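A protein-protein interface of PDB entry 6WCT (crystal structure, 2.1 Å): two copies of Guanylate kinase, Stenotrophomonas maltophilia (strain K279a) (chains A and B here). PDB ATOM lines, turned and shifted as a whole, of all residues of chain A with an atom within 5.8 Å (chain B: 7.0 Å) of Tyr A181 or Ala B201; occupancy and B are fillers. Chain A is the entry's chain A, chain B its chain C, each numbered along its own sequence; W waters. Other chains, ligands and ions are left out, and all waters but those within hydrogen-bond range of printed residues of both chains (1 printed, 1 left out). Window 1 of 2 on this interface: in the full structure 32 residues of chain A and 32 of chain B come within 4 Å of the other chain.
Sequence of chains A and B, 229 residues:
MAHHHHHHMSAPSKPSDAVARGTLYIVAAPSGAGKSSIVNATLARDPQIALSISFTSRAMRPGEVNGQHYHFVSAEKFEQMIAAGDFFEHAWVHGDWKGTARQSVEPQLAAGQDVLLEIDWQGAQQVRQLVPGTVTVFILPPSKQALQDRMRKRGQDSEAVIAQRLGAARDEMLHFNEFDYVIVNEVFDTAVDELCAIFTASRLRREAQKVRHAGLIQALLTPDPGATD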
ATOM      1  N   VAL A 135      -2.046 -10.443  23.451  1.00  0.00           N
ATOM      2  CA  VAL A 135      -3.161 -10.023  22.609  1.00  0.00           C
ATOM      3  C   VAL A 135      -2.755 -10.297  21.164  1.00  0.00           C
ATOM      4  O   VAL A 135      -1.791  -9.710  20.671  1.00  0.00           O
ATOM      5  CB  VAL A 135      -3.491  -8.536  22.821  1.00  0.00           C
ATOM      6  CG1 VAL A 135      -4.568  -8.058  21.812  1.00  0.00           C
ATOM      7  CG2 VAL A 135      -3.960  -8.305  24.235  1.00  0.00           C
ATOM      8  N   THR A 136      -3.499 -11.164  20.468  1.00  0.00           N
ATOM      9  CA  THR A 136      -3.089 -11.620  19.137  1.00  0.00           C
ATOM     10  C   THR A 136      -4.130 -11.231  18.088  1.00  0.00           C
ATOM     11  O   THR A 136      -5.330 -11.401  18.310  1.00  0.00           O
ATOM     12  CB  THR A 136      -2.841 -13.133  19.124  1.00  0.00           C
ATOM     13  OG1 THR A 136      -4.071 -13.809  19.356  1.00  0.00           O
ATOM     14  CG2 THR A 136      -1.834 -13.556  20.251  1.00  0.00           C
ATOM     15  N   VAL A 137      -3.660 -10.696  16.959  1.00  0.00           N
ATOM     16  CA  VAL A 137      -4.503 -10.169  15.888  1.00  0.00           C
ATOM     17  C   VAL A 137      -4.065 -10.771  14.557  1.00  0.00           C
ATOM     18  O   VAL A 137      -2.870 -10.809  14.255  1.00  0.00           O
ATOM     19  CB  VAL A 137      -4.414  -8.631  15.800  1.00  0.00           C
ATOM     20  CG1 VAL A 137      -5.372  -8.096  14.706  1.00  0.00           C
ATOM     21  CG2 VAL A 137      -4.644  -7.968  17.180  1.00  0.00           C
ATOM     22  N   PHE A 138      -5.024 -11.185  13.728  1.00  0.00           N
ATOM     23  CA  PHE A 138      -4.695 -11.657  12.390  1.00  0.00           C
ATOM     24  C   PHE A 138      -5.281 -10.707  11.356  1.00  0.00           C
ATOM     25  O   PHE A 138      -6.436 -10.288  11.467  1.00  0.00           O
ATOM     26  CB  PHE A 138      -5.211 -13.080  12.109  1.00  0.00           C
ATOM     27  CG  PHE A 138      -4.426 -13.786  11.025  1.00  0.00           C
ATOM     28  CD1 PHE A 138      -4.725 -13.594   9.692  1.00  0.00           C
ATOM     29  CD2 PHE A 138      -3.366 -14.619  11.350  1.00  0.00           C
ATOM     30  CE1 PHE A 138      -3.984 -14.224   8.705  1.00  0.00           C
ATOM     31  CE2 PHE A 138      -2.627 -15.254  10.370  1.00  0.00           C
ATOM     32  CZ  PHE A 138      -2.935 -15.054   9.046  1.00  0.00           C
ATOM     33  N   ILE A 139      -4.481 -10.367  10.351  1.00  0.00           N
ATOM     34  CA  ILE A 139      -4.918  -9.444   9.303  1.00  0.00           C
ATOM     35  C   ILE A 139      -5.028 -10.238   8.016  1.00  0.00           C
ATOM     36  O   ILE A 139      -4.071 -10.900   7.595  1.00  0.00           O
ATOM     37  CB  ILE A 139      -3.981  -8.233   9.172  1.00  0.00           C
ATOM     38  CG1 ILE A 139      -3.976  -7.458  10.505  1.00  0.00           C
ATOM     39  CG2 ILE A 139      -4.407  -7.346   8.016  1.00  0.00           C
ATOM     40  CD1 ILE A 139      -3.194  -6.161  10.506  1.00  0.00           C
ATOM     41  N   PHE A 176      -5.541 -18.870  10.995  1.00  0.00           N
ATOM     42  CA  PHE A 176      -6.111 -17.621  11.493  1.00  0.00           C
ATOM     43  C   PHE A 176      -6.959 -17.847  12.732  1.00  0.00           C
ATOM     44  O   PHE A 176      -7.100 -16.943  13.560  1.00  0.00           O
ATOM     45  CB  PHE A 176      -6.973 -16.952  10.407  1.00  0.00           C
ATOM     46  CG  PHE A 176      -8.371 -17.504  10.341  1.00  0.00           C
ATOM     47  CD1 PHE A 176      -8.619 -18.689   9.668  1.00  0.00           C
ATOM     48  CD2 PHE A 176      -9.419 -16.883  11.008  1.00  0.00           C
ATOM     49  CE1 PHE A 176      -9.884 -19.246   9.631  1.00  0.00           C
ATOM     50  CE2 PHE A 176     -10.687 -17.436  10.988  1.00  0.00           C
ATOM     51  CZ  PHE A 176     -10.926 -18.615  10.298  1.00  0.00           C
ATOM     52  N   PHE A 179      -6.182 -16.852  16.604  1.00  0.00           N
ATOM     53  CA  PHE A 179      -5.984 -15.470  17.005  1.00  0.00           C
ATOM     54  C   PHE A 179      -7.254 -14.868  17.606  1.00  0.00           C
ATOM     55  O   PHE A 179      -8.374 -15.292  17.300  1.00  0.00           O
ATOM     56  CB  PHE A 179      -5.482 -14.661  15.800  1.00  0.00           C
ATOM     57  CG  PHE A 179      -4.074 -15.040  15.385  1.00  0.00           C
ATOM     58  CD1 PHE A 179      -3.832 -16.221  14.690  1.00  0.00           C
ATOM     59  CD2 PHE A 179      -2.995 -14.258  15.741  1.00  0.00           C
ATOM     60  CE1 PHE A 179      -2.542 -16.594  14.334  1.00  0.00           C
ATOM     61  CE2 PHE A 179      -1.685 -14.623  15.384  1.00  0.00           C
ATOM     62  CZ  PHE A 179      -1.463 -15.793  14.689  1.00  0.00           C
ATOM     63  N   ASP A 180      -7.069 -13.890  18.511  1.00  0.00           N
ATOM     64  CA  ASP A 180      -8.232 -13.329  19.212  1.00  0.00           C
ATOM     65  C   ASP A 180      -9.074 -12.445  18.296  1.00  0.00           C
ATOM     66  O   ASP A 180     -10.309 -12.415  18.404  1.00  0.00           O
ATOM     67  CB  ASP A 180      -7.788 -12.519  20.421  1.00  0.00           C
ATOM     68  CG  ASP A 180      -6.930 -13.340  21.386  1.00  0.00           C
ATOM     69  OD1 ASP A 180      -7.413 -14.397  21.839  1.00  0.00           O
ATOM     70  OD2 ASP A 180      -5.799 -12.906  21.701  1.00  0.00           O
ATOM     71  N   TYR A 181      -8.422 -11.691  17.426  1.00  0.00           N
ATOM     72  CA  TYR A 181      -9.092 -10.701  16.585  1.00  0.00           C
ATOM     73  C   TYR A 181      -8.703 -10.946  15.144  1.00  0.00           C
ATOM     74  O   TYR A 181      -7.642 -11.507  14.862  1.00  0.00           O
ATOM     75  CB  TYR A 181      -8.707  -9.258  16.950  1.00  0.00           C
ATOM     76  CG  TYR A 181      -9.074  -8.906  18.354  1.00  0.00           C
ATOM     77  CD1 TYR A 181     -10.332  -8.403  18.663  1.00  0.00           C
ATOM     78  CD2 TYR A 181      -8.171  -9.105  19.380  1.00  0.00           C
ATOM     79  CE1 TYR A 181     -10.673  -8.100  19.976  1.00  0.00           C
ATOM     80  CE2 TYR A 181      -8.490  -8.802  20.672  1.00  0.00           C
ATOM     81  CZ  TYR A 181      -9.734  -8.299  20.974  1.00  0.00           C
ATOM     82  OH  TYR A 181     -10.019  -8.026  22.290  1.00  0.00           O
ATOM     83  N   VAL A 182      -9.586 -10.533  14.237  1.00  0.00           N
ATOM     84  CA  VAL A 182      -9.344 -10.642  12.812  1.00  0.00           C
ATOM     85  C   VAL A 182      -9.686  -9.294  12.207  1.00  0.00           C
ATOM     86  O   VAL A 182     -10.755  -8.750  12.490  1.00  0.00           O
ATOM     87  CB  VAL A 182     -10.170 -11.778  12.181  1.00  0.00           C
ATOM     88  CG1 VAL A 182     -10.015 -11.789  10.675  1.00  0.00           C
ATOM     89  CG2 VAL A 182      -9.723 -13.145  12.781  1.00  0.00           C
ATOM     90  N   ILE A 183      -8.744  -8.715  11.470  1.00  0.00           N
ATOM     91  CA  ILE A 183      -8.958  -7.477  10.722  1.00  0.00           C
ATOM     92  C   ILE A 183      -8.888  -7.808   9.239  1.00  0.00           C
ATOM     93  O   ILE A 183      -7.939  -8.465   8.799  1.00  0.00           O
ATOM     94  CB  ILE A 183      -7.911  -6.412  11.090  1.00  0.00           C
ATOM     95  CG1 ILE A 183      -8.049  -5.994  12.563  1.00  0.00           C
ATOM     96  CG2 ILE A 183      -7.998  -5.207  10.139  1.00  0.00           C
ATOM     97  CD1 ILE A 183      -6.926  -5.005  13.023  1.00  0.00           C
ATOM     98  N   GLU A 194      -8.974   0.271  13.345  1.00  0.00           N
ATOM     99  CA  GLU A 194      -9.406  -0.953  14.012  1.00  0.00           C
ATOM    100  C   GLU A 194      -8.288  -1.549  14.858  1.00  0.00           C
ATOM    101  O   GLU A 194      -8.527  -2.017  15.974  1.00  0.00           O
ATOM    102  CB  GLU A 194      -9.916  -1.949  12.962  1.00  0.00           C
ATOM    103  CG  GLU A 194     -11.188  -1.432  12.235  1.00  0.00           C
ATOM    104  CD  GLU A 194     -11.822  -2.441  11.275  1.00  0.00           C
ATOM    105  OE1 GLU A 194     -11.122  -3.361  10.800  1.00  0.00           O
ATOM    106  OE2 GLU A 194     -13.037  -2.308  10.999  1.00  0.00           O
ATOM    107  N   ALA A 197      -8.142   0.554  17.905  1.00  0.00           N
ATOM    108  CA  ALA A 197      -9.199   0.232  18.864  1.00  0.00           C
ATOM    109  C   ALA A 197      -8.860  -1.020  19.665  1.00  0.00           C
ATOM    110  O   ALA A 197      -9.109  -1.074  20.872  1.00  0.00           O
ATOM    111  CB  ALA A 197     -10.540   0.065  18.159  1.00  0.00           C
ATOM    112  N   ILE A 198      -8.284  -2.033  19.011  1.00  0.00           N
ATOM    113  CA  ILE A 198      -7.901  -3.263  19.708  1.00  0.00           C
ATOM    114  C   ILE A 198      -6.841  -2.970  20.764  1.00  0.00           C
ATOM    115  O   ILE A 198      -6.924  -3.451  21.896  1.00  0.00           O
ATOM    116  CB  ILE A 198      -7.407  -4.318  18.705  1.00  0.00           C
ATOM    117  CG1 ILE A 198      -8.557  -4.801  17.809  1.00  0.00           C
ATOM    118  CG2 ILE A 198      -6.689  -5.491  19.441  1.00  0.00           C
ATOM    119  CD1 ILE A 198      -8.089  -5.764  16.674  1.00  0.00           C
ATOM    120  N   ALA A 201      -8.498  -0.978  23.634  1.00  0.00           N
ATOM    121  CA  ALA A 201      -9.372  -1.807  24.456  1.00  0.00           C
ATOM    122  C   ALA A 201      -8.579  -2.716  25.379  1.00  0.00           C
ATOM    123  O   ALA A 201      -9.011  -2.986  26.506  1.00  0.00           O
ATOM    124  CB  ALA A 201     -10.289  -2.650  23.575  1.00  0.00           C
ATOM    125  N   TYR B  25     -24.041  -5.312  24.431  1.00  0.00           N
ATOM    126  CA  TYR B  25     -23.118  -4.561  25.274  1.00  0.00           C
ATOM    127  C   TYR B  25     -23.817  -4.162  26.556  1.00  0.00           C
ATOM    128  O   TYR B  25     -24.980  -3.744  26.528  1.00  0.00           O
ATOM    129  CB  TYR B  25     -22.592  -3.303  24.582  1.00  0.00           C
ATOM    130  CG  TYR B  25     -21.830  -3.558  23.306  1.00  0.00           C
ATOM    131  CD1 TYR B  25     -20.505  -3.943  23.338  1.00  0.00           C
ATOM    132  CD2 TYR B  25     -22.431  -3.369  22.063  1.00  0.00           C
ATOM    133  CE1 TYR B  25     -19.796  -4.165  22.173  1.00  0.00           C
ATOM    134  CE2 TYR B  25     -21.726  -3.584  20.886  1.00  0.00           C
ATOM    135  CZ  TYR B  25     -20.409  -3.983  20.953  1.00  0.00           C
ATOM    136  OH  TYR B  25     -19.692  -4.204  19.804  1.00  0.00           O
ATOM    137  N   TYR B 181     -14.389  -4.938  31.096  1.00  0.00           N
ATOM    138  CA  TYR B 181     -13.620  -3.719  30.912  1.00  0.00           C
ATOM    139  C   TYR B 181     -13.967  -2.735  32.017  1.00  0.00           C
ATOM    140  O   TYR B 181     -15.066  -2.767  32.575  1.00  0.00           O
ATOM    141  CB  TYR B 181     -13.885  -3.074  29.548  1.00  0.00           C
ATOM    142  CG  TYR B 181     -13.495  -3.920  28.355  1.00  0.00           C
ATOM    143  CD1 TYR B 181     -12.231  -3.831  27.799  1.00  0.00           C
ATOM    144  CD2 TYR B 181     -14.403  -4.794  27.774  1.00  0.00           C
ATOM    145  CE1 TYR B 181     -11.880  -4.610  26.695  1.00  0.00           C
ATOM    146  CE2 TYR B 181     -14.068  -5.567  26.706  1.00  0.00           C
ATOM    147  CZ  TYR B 181     -12.810  -5.465  26.156  1.00  0.00           C
ATOM    148  OH  TYR B 181     -12.508  -6.236  25.067  1.00  0.00           O
ATOM    149  N   LEU B 195     -14.874   4.053  25.338  1.00  0.00           N
ATOM    150  CA  LEU B 195     -16.061   3.238  25.129  1.00  0.00           C
ATOM    151  C   LEU B 195     -16.219   2.887  23.653  1.00  0.00           C
ATOM    152  O   LEU B 195     -16.520   1.736  23.309  1.00  0.00           O
ATOM    153  CB  LEU B 195     -17.312   3.957  25.653  1.00  0.00           C
ATOM    154  CG  LEU B 195     -18.543   3.038  25.603  1.00  0.00           C
ATOM    155  CD1 LEU B 195     -18.277   1.775  26.408  1.00  0.00           C
ATOM    156  CD2 LEU B 195     -19.821   3.721  26.092  1.00  0.00           C
ATOM    157  N   CYS B 196     -15.974   3.845  22.763  1.00  0.00           N
ATOM    158  CA  CYS B 196     -16.026   3.532  21.337  1.00  0.00           C
ATOM    159  C   CYS B 196     -14.985   2.491  20.957  1.00  0.00           C
ATOM    160  O   CYS B 196     -15.287   1.548  20.220  1.00  0.00           O
ATOM    161  CB  CYS B 196     -15.848   4.798  20.507  1.00  0.00           C
ATOM    162  SG  CYS B 196     -17.278   5.904  20.624  1.00  0.00           S
ATOM    163  N   ALA B 197     -13.769   2.603  21.488  1.00  0.00           N
ATOM    164  CA  ALA B 197     -12.769   1.591  21.169  1.00  0.00           C
ATOM    165  C   ALA B 197     -13.251   0.205  21.574  1.00  0.00           C
ATOM    166  O   ALA B 197     -13.034  -0.769  20.848  1.00  0.00           O
ATOM    167  CB  ALA B 197     -11.439   1.906  21.849  1.00  0.00           C
ATOM    168  N   ILE B 198     -13.905   0.097  22.731  1.00  0.00           N
ATOM    169  CA  ILE B 198     -14.391  -1.203  23.192  1.00  0.00           C
ATOM    170  C   ILE B 198     -15.421  -1.767  22.217  1.00  0.00           C
ATOM    171  O   ILE B 198     -15.380  -2.953  21.855  1.00  0.00           O
ATOM    172  CB  ILE B 198     -14.955  -1.073  24.622  1.00  0.00           C
ATOM    173  CG1 ILE B 198     -13.822  -0.783  25.608  1.00  0.00           C
ATOM    174  CG2 ILE B 198     -15.772  -2.299  25.018  1.00  0.00           C
ATOM    175  CD1 ILE B 198     -14.289  -0.518  27.060  1.00  0.00           C
ATOM    176  N   PHE B 199     -16.348  -0.929  21.760  1.00  0.00           N
ATOM    177  CA  PHE B 199     -17.352  -1.405  20.818  1.00  0.00           C
ATOM    178  C   PHE B 199     -16.705  -1.828  19.505  1.00  0.00           C
ATOM    179  O   PHE B 199     -16.986  -2.909  18.978  1.00  0.00           O
ATOM    180  CB  PHE B 199     -18.405  -0.320  20.589  1.00  0.00           C
ATOM    181  CG  PHE B 199     -19.238  -0.022  21.813  1.00  0.00           C
ATOM    182  CD1 PHE B 199     -19.189  -0.845  22.919  1.00  0.00           C
ATOM    183  CD2 PHE B 199     -20.064   1.072  21.855  1.00  0.00           C
ATOM    184  CE1 PHE B 199     -19.954  -0.579  24.041  1.00  0.00           C
ATOM    185  CE2 PHE B 199     -20.831   1.339  22.972  1.00  0.00           C
ATOM    186  CZ  PHE B 199     -20.778   0.511  24.062  1.00  0.00           C
ATOM    187  N   THR B 200     -15.781  -1.012  18.999  1.00  0.00           N
ATOM    188  CA  THR B 200     -15.088  -1.333  17.755  1.00  0.00           C
ATOM    189  C   THR B 200     -14.302  -2.630  17.872  1.00  0.00           C
ATOM    190  O   THR B 200     -14.419  -3.517  17.018  1.00  0.00           O
ATOM    191  CB  THR B 200     -14.162  -0.182  17.375  1.00  0.00           C
ATOM    192  OG1 THR B 200     -14.951   0.989  17.135  1.00  0.00           O
ATOM    193  CG2 THR B 200     -13.320  -0.533  16.135  1.00  0.00           C
ATOM    194  N   ALA B 201     -13.489  -2.759  18.926  1.00  0.00           N
ATOM    195  CA  ALA B 201     -12.672  -3.956  19.083  1.00  0.00           C
ATOM    196  C   ALA B 201     -13.538  -5.203  19.205  1.00  0.00           C
ATOM    197  O   ALA B 201     -13.169  -6.283  18.720  1.00  0.00           O
ATOM    198  CB  ALA B 201     -11.751  -3.816  20.304  1.00  0.00           C
ATOM    199  N   SER B 202     -14.696  -5.079  19.851  1.00  0.00           N
ATOM    200  CA  SER B 202     -15.512  -6.261  20.103  1.00  0.00           C
ATOM    201  C   SER B 202     -16.069  -6.839  18.808  1.00  0.00           C
ATOM    202  O   SER B 202     -16.262  -8.057  18.710  1.00  0.00           O
ATOM    203  CB  SER B 202     -16.643  -5.915  21.076  1.00  0.00           C
ATOM    204  OG  SER B 202     -16.086  -5.446  22.291  1.00  0.00           O
ATOM    205  N   ARG B 203     -16.321  -5.989  17.808  1.00  0.00           N
ATOM    206  CA  ARG B 203     -16.786  -6.468  16.512  1.00  0.00           C
ATOM    207  C   ARG B 203     -15.692  -7.160  15.716  1.00  0.00           C
ATOM    208  O   ARG B 203     -16.001  -7.894  14.777  1.00  0.00           O
ATOM    209  CB  ARG B 203     -17.344  -5.311  15.687  1.00  0.00           C
ATOM    210  CG  ARG B 203     -18.433  -4.581  16.397  1.00  0.00           C
ATOM    211  CD  ARG B 203     -19.137  -3.595  15.480  1.00  0.00           C
ATOM    212  NE  ARG B 203     -20.076  -2.787  16.240  1.00  0.00           N
ATOM    213  CZ  ARG B 203     -19.809  -1.565  16.681  1.00  0.00           C
ATOM    214  NH1 ARG B 203     -18.632  -1.018  16.415  1.00  0.00           N
ATOM    215  NH2 ARG B 203     -20.718  -0.889  17.380  1.00  0.00           N
ATOM    216  N   LEU B 204     -14.429  -6.961  16.077  1.00  0.00           N
ATOM    217  CA  LEU B 204     -13.325  -7.595  15.370  1.00  0.00           C
ATOM    218  C   LEU B 204     -12.965  -8.949  15.967  1.00  0.00           C
ATOM    219  O   LEU B 204     -12.038  -9.602  15.477  1.00  0.00           O
ATOM    220  CB  LEU B 204     -12.104  -6.681  15.395  1.00  0.00           C
ATOM    221  CG  LEU B 204     -12.367  -5.285  14.841  1.00  0.00           C
ATOM    222  CD1 LEU B 204     -11.188  -4.406  15.156  1.00  0.00           C
ATOM    223  CD2 LEU B 204     -12.658  -5.339  13.337  1.00  0.00           C
ATOM    224  N   ARG B 205     -13.663  -9.369  17.022  1.00  0.00           N
ATOM    225  CA  ARG B 205     -13.377 -10.655  17.645  1.00  0.00           C
ATOM    226  C   ARG B 205     -13.569 -11.784  16.640  1.00  0.00           C
ATOM    227  O   ARG B 205     -14.422 -11.718  15.751  1.00  0.00           O
ATOM    228  CB  ARG B 205     -14.266 -10.875  18.880  1.00  0.00           C
ATOM    229  CG  ARG B 205     -13.813 -10.029  20.070  1.00  0.00           C
ATOM    230  CD  ARG B 205     -14.683 -10.244  21.311  1.00  0.00           C
ATOM    231  NE  ARG B 205     -16.076  -9.927  21.034  1.00  0.00           N
ATOM    232  CZ  ARG B 205     -17.072 -10.138  21.885  1.00  0.00           C
ATOM    233  NH1 ARG B 205     -16.828 -10.668  23.074  1.00  0.00           N
ATOM    234  NH2 ARG B 205     -18.311  -9.822  21.547  1.00  0.00           N
ATOM    235  N   ARG B 206     -12.754 -12.829  16.797  1.00  0.00           N
ATOM    236  CA  ARG B 206     -12.646 -13.873  15.785  1.00  0.00           C
ATOM    237  C   ARG B 206     -13.998 -14.469  15.402  1.00  0.00           C
ATOM    238  O   ARG B 206     -14.328 -14.576  14.217  1.00  0.00           O
ATOM    239  CB  ARG B 206     -11.725 -14.973  16.298  1.00  0.00           C
ATOM    240  CG  ARG B 206     -11.724 -16.176  15.407  1.00  0.00           C
ATOM    241  CD  ARG B 206     -11.039 -17.347  16.089  1.00  0.00           C
ATOM    242  NE  ARG B 206     -11.713 -17.746  17.317  1.00  0.00           N
ATOM    243  CZ  ARG B 206     -11.215 -17.528  18.529  1.00  0.00           C
ATOM    244  NH1 ARG B 206     -10.048 -16.926  18.646  1.00  0.00           N
ATOM    245  NH2 ARG B 206     -11.867 -17.913  19.613  1.00  0.00           N
ATOM    246  N   GLN B 209     -16.086 -12.318  13.266  1.00  0.00           N
ATOM    247  CA  GLN B 209     -15.521 -12.104  11.940  1.00  0.00           C
ATOM    248  C   GLN B 209     -15.613 -13.359  11.074  1.00  0.00           C
ATOM    249  O   GLN B 209     -15.716 -13.257   9.848  1.00  0.00           O
ATOM    250  CB  GLN B 209     -14.076 -11.636  12.070  1.00  0.00           C
ATOM    251  CG  GLN B 209     -13.922 -10.217  12.655  1.00  0.00           C
ATOM    252  CD  GLN B 209     -14.308  -9.116  11.683  1.00  0.00           C
ATOM    253  OE1 GLN B 209     -15.451  -9.036  11.257  1.00  0.00           O
ATOM    254  NE2 GLN B 209     -13.345  -8.266  11.323  1.00  0.00           N
HETATM  255  O   HOH W   1     -12.037  -5.644   9.579  1.00  0.00           O
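The guanidinium group of Arg B206 lies within hydrogen-bond range of the backbone carbonyl oxygen of Phe A179 (2.7 Å).
The backbone carbonyl oxygen (O) of Asp A180 sits at hydrogen-bond distance from the backbone NH (N) of Arg B206.
N of Val A182 lies within hydrogen-bond range of O of Leu B204, 2.9 Å away.
The side-chain amide nitrogen of Gln B209 sits at hydrogen-bond distance from the backbone carbonyl oxygen of Val A182 (2.9 Å).
The backbone NH of Asp A180 sits at hydrogen-bond distance from the backbone carbonyl oxygen of Thr A136 (3.0 Å).
The backbone NH (N) of Tyr A181 is in hydrogen-bond range of the backbone carbonyl oxygen (O) of Thr A136 (3.2 Å).
O of Tyr A181 is in hydrogen-bond range of N of Phe A138 (2.9 Å).
O of Cys B196 sits at hydrogen-bond distance from OG1 of Thr B200, at 3.2 Å.
O of Ser B202 is in hydrogen-bond range of NE of Arg B205, at 3.0 Å.
Asp A180 touches Arg B205.
CE1 of Tyr A181 touches O of Ala B201 (3.3 Å).
Leu B204 touches Tyr A181 (O to CA, 3.3 Å).
Tyr A181 touches Arg B205 (CE1 to CG, 3.7 Å).
Glu A194 touches Leu B204.
Ala A197 touches Ala B197.
Ile A198 touches Ala B201.
CD1 of Leu B204 touches CD1 of Ile A198, at 3.7 Å.
Ala A201 touches Tyr B181.
CB of Ala A201 touches CB of Ala B201, at 3.8 Å.
Tyr A181 touches just these residues of chain B: Ala B201, Leu B204 and Arg B205.
Of chain A, only Tyr A181, Ala A197, Ile A198 and Ala A201 come within 4 Å of Ala B201.
Of the printed residues of chain B, Glu A194 touches Leu B204.
Of the printed residues of chain A, Leu B204 touches Tyr A181 (3.3 Å), Val A182 (2.9 Å), Glu A194 (3.5 Å) and Ile A198 (3.7 Å).
Printed residues of chain B within 4 Å of Val A182: Leu B204 and Gln B209.
Of the printed residues of chain A, Tyr B181 touches Ala A201 (3.3 Å).
Val A137 touches none of the printed residues of chain B.
The nearest residue of chain B that does not touch Tyr A181 is Tyr B181 (4.1 Å).
The nearest printed residue of chain B that does not touch Asp A180 is Leu B204 (4.4 Å).
Of the 15 printed residues of chain A, 8 touch a printed residue of chain B.
Hydrophobic or aromatic side chains of chain A that line the printed part of chain B: Tyr A181, Val A182, Ala A197, Ile A198 and Ala A201.
Along chain A the printed residues that touch a printed residue of chain B span positions 179 to 201.
Hydrophobic or aromatic side chains of chain B that line the printed part of chain A: Tyr B181, Ala B197, Ala B201 and Leu B204.
Among the printed residues, 16 pairs touch across the chains.
Tyr A181 touches Ala B201, and with the chains exchanged Ala A201 touches Tyr B181.
Ala A197 touches its own counterpart, Ala B197.
Ile A198 touches Ala B201, but with the chains exchanged Ala A201 does not touch Ile B198 (4.4 Å).
Ala B201 touches its own counterpart, Ala A201.
4 positions are printed for both chains.
Water W1 bridges the side-chain carboxylate of Glu A194 and the side-chain amide nitrogen of Gln B209.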
